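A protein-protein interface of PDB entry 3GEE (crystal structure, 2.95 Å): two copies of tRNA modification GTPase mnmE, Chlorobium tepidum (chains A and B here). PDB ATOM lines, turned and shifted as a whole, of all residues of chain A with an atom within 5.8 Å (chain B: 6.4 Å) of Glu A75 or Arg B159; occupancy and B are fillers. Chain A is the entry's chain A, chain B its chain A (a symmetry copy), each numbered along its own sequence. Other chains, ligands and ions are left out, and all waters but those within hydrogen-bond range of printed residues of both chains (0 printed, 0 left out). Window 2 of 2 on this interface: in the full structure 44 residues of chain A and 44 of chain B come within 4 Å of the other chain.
Among the printed residues, merely in contact across the chains: Met A76 with Val B162, Val A77 with Arg B159, Val A77 with Val B162, Arg A110 with Tyr B158 and Arg A110 with Arg B159.
No position is printed for both chains.
Printed residues of chain A that touch a printed residue of chain B: Glu A75, Met A76, Val A77 and Arg A110.
Hydrophobic or aromatic side chains of chain A within 4 Å of the printed part of chain B: Met A76 and Val A77.
Printed residues of chain B that touch a printed residue of chain A: Tyr B158, Arg B159 and Val B162.
Among the printed residues, 8 pairs touch across the chains.
Among the printed residues, Asp or Glu carboxylates within 4 Å of a Lys or Arg side-chain nitrogen of the other chain: Glu A75 with Arg B159.
Of chain B, only Arg B159 (3.1 Å) comes within 4 Å of Glu A75.
Of the printed residues of chain B, Val A77 touches Tyr B158, Arg B159 and Val B162.
Of the printed residues of chain B, Arg A110 touches Tyr B158 and Arg B159.
Thr B154 touches none of the printed residues of chain A.
Of chain A, only Glu A75, Met A76, Val A77 and Arg A110 come within 4 Å of Arg B159.
The nearest residue of chain B that does not touch Glu A75 is Tyr B158 (6.0 Å).
The nearest printed residue of chain A that does not touch Arg B159 is Asp A72 (6.4 Å).
The nearest printed residue of chain B that does not touch Arg A110 is Glu B155 (6.5 Å).
O of Leu A70 is in hydrogen-bond range of N of Val A77 (2.8 Å).
OD2 of Asp A72 lies within salt-bridge range of NH1 of Arg A110 (3.5 Å).
The guanidinium group (NH2) of Arg A110 is in salt-bridge range of the side-chain carboxylate (OE2) of Glu A75, 2.7 Å away.
OH of Tyr B158 is in hydrogen-bond range of O of Val A77 (2.5 Å).
The guanidinium group (NH2) of Arg B159 is in hydrogen-bond range of the backbone carbonyl oxygen (O) of Met A76 (2.8 Å).
The guanidinium group (NE) of Arg B159 lies within salt-bridge range of the side-chain carboxylate (OE2) of Glu A75, 3.1 Å away.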
ATOM      1  N   LEU A  70      22.693  34.850 -12.267  1.00  0.00           N
ATOM      2  CA  LEU A  70      21.949  35.546 -13.308  1.00  0.00           C
ATOM      3  C   LEU A  70      20.463  35.462 -12.996  1.00  0.00           C
ATOM      4  O   LEU A  70      20.002  34.482 -12.415  1.00  0.00           O
ATOM      5  CB  LEU A  70      22.264  34.963 -14.681  1.00  0.00           C
ATOM      6  CG  LEU A  70      23.687  35.224 -15.177  1.00  0.00           C
ATOM      7  CD1 LEU A  70      24.024  34.333 -16.357  1.00  0.00           C
ATOM      8  CD2 LEU A  70      23.866  36.694 -15.536  1.00  0.00           C
ATOM      9  N   TYR A  71      19.719  36.497 -13.362  1.00  0.00           N
ATOM     10  CA  TYR A  71      18.313  36.588 -12.997  1.00  0.00           C
ATOM     11  C   TYR A  71      17.477  37.165 -14.117  1.00  0.00           C
ATOM     12  O   TYR A  71      17.890  38.109 -14.794  1.00  0.00           O
ATOM     13  CB  TYR A  71      18.135  37.456 -11.746  1.00  0.00           C
ATOM     14  CG  TYR A  71      18.211  36.698 -10.443  1.00  0.00           C
ATOM     15  CD1 TYR A  71      19.431  36.487  -9.805  1.00  0.00           C
ATOM     16  CD2 TYR A  71      17.058  36.197  -9.842  1.00  0.00           C
ATOM     17  CE1 TYR A  71      19.501  35.789  -8.604  1.00  0.00           C
ATOM     18  CE2 TYR A  71      17.118  35.498  -8.639  1.00  0.00           C
ATOM     19  CZ  TYR A  71      18.343  35.300  -8.027  1.00  0.00           C
ATOM     20  OH  TYR A  71      18.416  34.609  -6.841  1.00  0.00           O
ATOM     21  N   ASP A  72      16.296  36.587 -14.307  1.00  0.00           N
ATOM     22  CA  ASP A  72      15.293  37.175 -15.176  1.00  0.00           C
ATOM     23  C   ASP A  72      14.214  37.760 -14.275  1.00  0.00           C
ATOM     24  O   ASP A  72      13.063  37.335 -14.309  1.00  0.00           O
ATOM     25  CB  ASP A  72      14.724  36.135 -16.145  1.00  0.00           C
ATOM     26  CG  ASP A  72      14.088  36.768 -17.376  1.00  0.00           C
ATOM     27  OD1 ASP A  72      13.001  37.373 -17.251  1.00  0.00           O
ATOM     28  OD2 ASP A  72      14.672  36.656 -18.475  1.00  0.00           O
ATOM     29  N   GLY A  73      14.621  38.733 -13.461  1.00  0.00           N
ATOM     30  CA  GLY A  73      13.760  39.353 -12.465  1.00  0.00           C
ATOM     31  C   GLY A  73      13.203  38.330 -11.496  1.00  0.00           C
ATOM     32  O   GLY A  73      12.142  37.750 -11.745  1.00  0.00           O
ATOM     33  N   GLU A  74      13.919  38.104 -10.395  1.00  0.00           N
ATOM     34  CA  GLU A  74      13.514  37.127  -9.361  1.00  0.00           C
ATOM     35  C   GLU A  74      13.485  35.675  -9.842  1.00  0.00           C
ATOM     36  O   GLU A  74      13.093  34.781  -9.092  1.00  0.00           O
ATOM     37  CB  GLU A  74      12.167  37.500  -8.713  1.00  0.00           C
ATOM     38  CG  GLU A  74      12.280  38.215  -7.371  1.00  0.00           C
ATOM     39  CD  GLU A  74      12.551  39.705  -7.501  1.00  0.00           C
ATOM     40  OE1 GLU A  74      11.751  40.498  -6.959  1.00  0.00           O
ATOM     41  OE2 GLU A  74      13.557  40.089  -8.139  1.00  0.00           O
ATOM     42  N   GLU A  75      13.895  35.450 -11.089  1.00  0.00           N
ATOM     43  CA  GLU A  75      13.984  34.106 -11.635  1.00  0.00           C
ATOM     44  C   GLU A  75      15.445  33.743 -11.848  1.00  0.00           C
ATOM     45  O   GLU A  75      16.083  34.207 -12.791  1.00  0.00           O
ATOM     46  CB  GLU A  75      13.182  33.986 -12.932  1.00  0.00           C
ATOM     47  CG  GLU A  75      13.171  32.580 -13.512  1.00  0.00           C
ATOM     48  CD  GLU A  75      11.792  32.128 -13.977  1.00  0.00           C
ATOM     49  OE1 GLU A  75      10.788  32.384 -13.267  1.00  0.00           O
ATOM     50  OE2 GLU A  75      11.718  31.493 -15.050  1.00  0.00           O
ATOM     51  N   MET A  76      15.970  32.919 -10.951  1.00  0.00           N
ATOM     52  CA  MET A  76      17.381  32.559 -10.974  1.00  0.00           C
ATOM     53  C   MET A  76      17.694  31.712 -12.201  1.00  0.00           C
ATOM     54  O   MET A  76      17.263  30.565 -12.304  1.00  0.00           O
ATOM     55  CB  MET A  76      17.756  31.829  -9.681  1.00  0.00           C
ATOM     56  CG  MET A  76      19.193  32.018  -9.256  1.00  0.00           C
ATOM     57  SD  MET A  76      20.229  30.592  -9.599  1.00  0.00           S
ATOM     58  CE  MET A  76      19.885  29.592  -8.155  1.00  0.00           C
ATOM     59  N   VAL A  77      18.426  32.294 -13.141  1.00  0.00           N
ATOM     60  CA  VAL A  77      18.762  31.607 -14.381  1.00  0.00           C
ATOM     61  C   VAL A  77      19.867  30.573 -14.169  1.00  0.00           C
ATOM     62  O   VAL A  77      19.724  29.415 -14.567  1.00  0.00           O
ATOM     63  CB  VAL A  77      19.106  32.606 -15.508  1.00  0.00           C
ATOM     64  CG1 VAL A  77      19.941  31.952 -16.610  1.00  0.00           C
ATOM     65  CG2 VAL A  77      17.825  33.205 -16.079  1.00  0.00           C
ATOM     66  N   ARG A 110      19.290  29.609 -22.170  1.00  0.00           N
ATOM     67  CA  ARG A 110      18.616  30.565 -21.308  1.00  0.00           C
ATOM     68  C   ARG A 110      19.492  31.788 -21.057  1.00  0.00           C
ATOM     69  O   ARG A 110      19.004  32.926 -21.102  1.00  0.00           O
ATOM     70  CB  ARG A 110      18.240  29.915 -19.980  1.00  0.00           C
ATOM     71  CG  ARG A 110      16.760  29.728 -19.771  1.00  0.00           C
ATOM     72  CD  ARG A 110      16.073  31.068 -19.519  1.00  0.00           C
ATOM     73  NE  ARG A 110      14.949  30.931 -18.593  1.00  0.00           N
ATOM     74  CZ  ARG A 110      14.374  31.947 -17.954  1.00  0.00           C
ATOM     75  NH1 ARG A 110      14.808  33.193 -18.139  1.00  0.00           N
ATOM     76  NH2 ARG A 110      13.360  31.715 -17.126  1.00  0.00           N
ATOM     77  N   ALA B 152      19.257  18.236 -18.255  1.00  0.00           N
ATOM     78  CA  ALA B 152      17.853  18.634 -18.427  1.00  0.00           C
ATOM     79  C   ALA B 152      17.499  18.904 -19.883  1.00  0.00           C
ATOM     80  O   ALA B 152      18.270  19.531 -20.604  1.00  0.00           O
ATOM     81  CB  ALA B 152      17.535  19.851 -17.582  1.00  0.00           C
ATOM     82  N   THR B 154      13.896  19.552 -20.583  1.00  0.00           N
ATOM     83  CA  THR B 154      12.624  20.258 -20.467  1.00  0.00           C
ATOM     84  C   THR B 154      12.815  21.519 -19.631  1.00  0.00           C
ATOM     85  O   THR B 154      13.713  21.577 -18.791  1.00  0.00           O
ATOM     86  CB  THR B 154      11.547  19.391 -19.771  1.00  0.00           C
ATOM     87  OG1 THR B 154      11.897  18.005 -19.856  1.00  0.00           O
ATOM     88  CG2 THR B 154      10.187  19.615 -20.408  1.00  0.00           C
ATOM     89  N   GLU B 155      11.967  22.522 -19.858  1.00  0.00           N
ATOM     90  CA  GLU B 155      11.960  23.733 -19.034  1.00  0.00           C
ATOM     91  C   GLU B 155      11.711  23.394 -17.569  1.00  0.00           C
ATOM     92  O   GLU B 155      12.470  23.813 -16.690  1.00  0.00           O
ATOM     93  CB  GLU B 155      10.912  24.732 -19.530  1.00  0.00           C
ATOM     94  CG  GLU B 155      11.445  25.763 -20.523  1.00  0.00           C
ATOM     95  CD  GLU B 155      10.336  26.500 -21.292  1.00  0.00           C
ATOM     96  OE1 GLU B 155       9.128  26.347 -20.962  1.00  0.00           O
ATOM     97  OE2 GLU B 155      10.684  27.242 -22.243  1.00  0.00           O
ATOM     98  N   SER B 156      10.660  22.614 -17.319  1.00  0.00           N
ATOM     99  CA  SER B 156      10.288  22.213 -15.967  1.00  0.00           C
ATOM    100  C   SER B 156      11.363  21.367 -15.283  1.00  0.00           C
ATOM    101  O   SER B 156      11.487  21.396 -14.060  1.00  0.00           O
ATOM    102  CB  SER B 156       8.960  21.465 -15.979  1.00  0.00           C
ATOM    103  OG  SER B 156       9.093  20.223 -16.650  1.00  0.00           O
ATOM    104  N   ALA B 157      12.131  20.616 -16.071  1.00  0.00           N
ATOM    105  CA  ALA B 157      13.258  19.843 -15.544  1.00  0.00           C
ATOM    106  C   ALA B 157      14.408  20.766 -15.161  1.00  0.00           C
ATOM    107  O   ALA B 157      15.058  20.577 -14.130  1.00  0.00           O
ATOM    108  CB  ALA B 157      13.723  18.809 -16.558  1.00  0.00           C
ATOM    109  N   TYR B 158      14.646  21.761 -16.010  1.00  0.00           N
ATOM    110  CA  TYR B 158      15.655  22.794 -15.787  1.00  0.00           C
ATOM    111  C   TYR B 158      15.350  23.609 -14.525  1.00  0.00           C
ATOM    112  O   TYR B 158      16.208  23.764 -13.653  1.00  0.00           O
ATOM    113  CB  TYR B 158      15.745  23.695 -17.032  1.00  0.00           C
ATOM    114  CG  TYR B 158      16.303  25.081 -16.799  1.00  0.00           C
ATOM    115  CD1 TYR B 158      17.672  25.285 -16.647  1.00  0.00           C
ATOM    116  CD2 TYR B 158      15.460  26.192 -16.754  1.00  0.00           C
ATOM    117  CE1 TYR B 158      18.189  26.555 -16.437  1.00  0.00           C
ATOM    118  CE2 TYR B 158      15.967  27.470 -16.545  1.00  0.00           C
ATOM    119  CZ  TYR B 158      17.332  27.642 -16.386  1.00  0.00           C
ATOM    120  OH  TYR B 158      17.840  28.898 -16.181  1.00  0.00           O
ATOM    121  N   ARG B 159      14.119  24.107 -14.434  1.00  0.00           N
ATOM    122  CA  ARG B 159      13.678  24.913 -13.300  1.00  0.00           C
ATOM    123  C   ARG B 159      13.721  24.151 -11.980  1.00  0.00           C
ATOM    124  O   ARG B 159      13.974  24.737 -10.927  1.00  0.00           O
ATOM    125  CB  ARG B 159      12.274  25.455 -13.559  1.00  0.00           C
ATOM    126  CG  ARG B 159      12.258  26.661 -14.478  1.00  0.00           C
ATOM    127  CD  ARG B 159      12.196  27.949 -13.678  1.00  0.00           C
ATOM    128  NE  ARG B 159      13.165  28.937 -14.147  1.00  0.00           N
ATOM    129  CZ  ARG B 159      14.364  29.122 -13.603  1.00  0.00           C
ATOM    130  NH1 ARG B 159      14.752  28.387 -12.572  1.00  0.00           N
ATOM    131  NH2 ARG B 159      15.179  30.044 -14.091  1.00  0.00           N
ATOM    132  N   THR B 160      13.482  22.845 -12.048  1.00  0.00           N
ATOM    133  CA  THR B 160      13.520  21.983 -10.873  1.00  0.00           C
ATOM    134  C   THR B 160      14.944  21.845 -10.337  1.00  0.00           C
ATOM    135  O   THR B 160      15.159  21.888  -9.125  1.00  0.00           O
ATOM    136  CB  THR B 160      12.894  20.602 -11.172  1.00  0.00           C
ATOM    137  OG1 THR B 160      11.522  20.784 -11.532  1.00  0.00           O
ATOM    138  CG2 THR B 160      12.965  19.684  -9.959  1.00  0.00           C
ATOM    139  N   ALA B 161      15.912  21.699 -11.238  1.00  0.00           N
ATOM    140  CA  ALA B 161      17.311  21.587 -10.838  1.00  0.00           C
ATOM    141  C   ALA B 161      17.827  22.894 -10.242  1.00  0.00           C
ATOM    142  O   ALA B 161      18.591  22.880  -9.274  1.00  0.00           O
ATOM    143  CB  ALA B 161      18.173  21.154 -12.006  1.00  0.00           C
ATOM    144  N   VAL B 162      17.404  24.018 -10.820  1.00  0.00           N
ATOM    145  CA  VAL B 162      17.769  25.335 -10.303  1.00  0.00           C
ATOM    146  C   VAL B 162      17.340  25.460  -8.845  1.00  0.00           C
ATOM    147  O   VAL B 162      18.135  25.850  -7.994  1.00  0.00           O
ATOM    148  CB  VAL B 162      17.169  26.477 -11.149  1.00  0.00           C
ATOM    149  CG1 VAL B 162      17.296  27.808 -10.429  1.00  0.00           C
ATOM    150  CG2 VAL B 162      17.851  26.549 -12.509  1.00  0.00           C
ATOM    151  N   SER B 163      16.091  25.102  -8.566  1.00  0.00           N
ATOM    152  CA  SER B 163      15.565  25.093  -7.205  1.00  0.00           C
ATOM    153  C   SER B 163      16.421  24.235  -6.269  1.00  0.00           C
ATOM    154  O   SER B 163      16.765  24.661  -5.162  1.00  0.00           O
ATOM    155  CB  SER B 163      14.118  24.604  -7.199  1.00  0.00           C
ATOM    156  OG  SER B 163      13.652  24.416  -5.874  1.00  0.00           O
ATOM    157  N   GLN B 164      16.773  23.036  -6.725  1.00  0.00           N
ATOM    158  CA  GLN B 164      17.550  22.105  -5.913  1.00  0.00           C
ATOM    159  C   GLN B 164      18.995  22.575  -5.719  1.00  0.00           C
ATOM    160  O   GLN B 164      19.612  22.293  -4.686  1.00  0.00           O
ATOM    161  CB  GLN B 164      17.502  20.705  -6.527  1.00  0.00           C
ATOM    162  CG  GLN B 164      18.063  19.596  -5.637  1.00  0.00           C
ATOM    163  CD  GLN B 164      17.626  18.213  -6.083  1.00  0.00           C
ATOM    164  OE1 GLN B 164      16.434  17.955  -6.255  1.00  0.00           O
ATOM    165  NE2 GLN B 164      18.586  17.314  -6.267  1.00  0.00           N
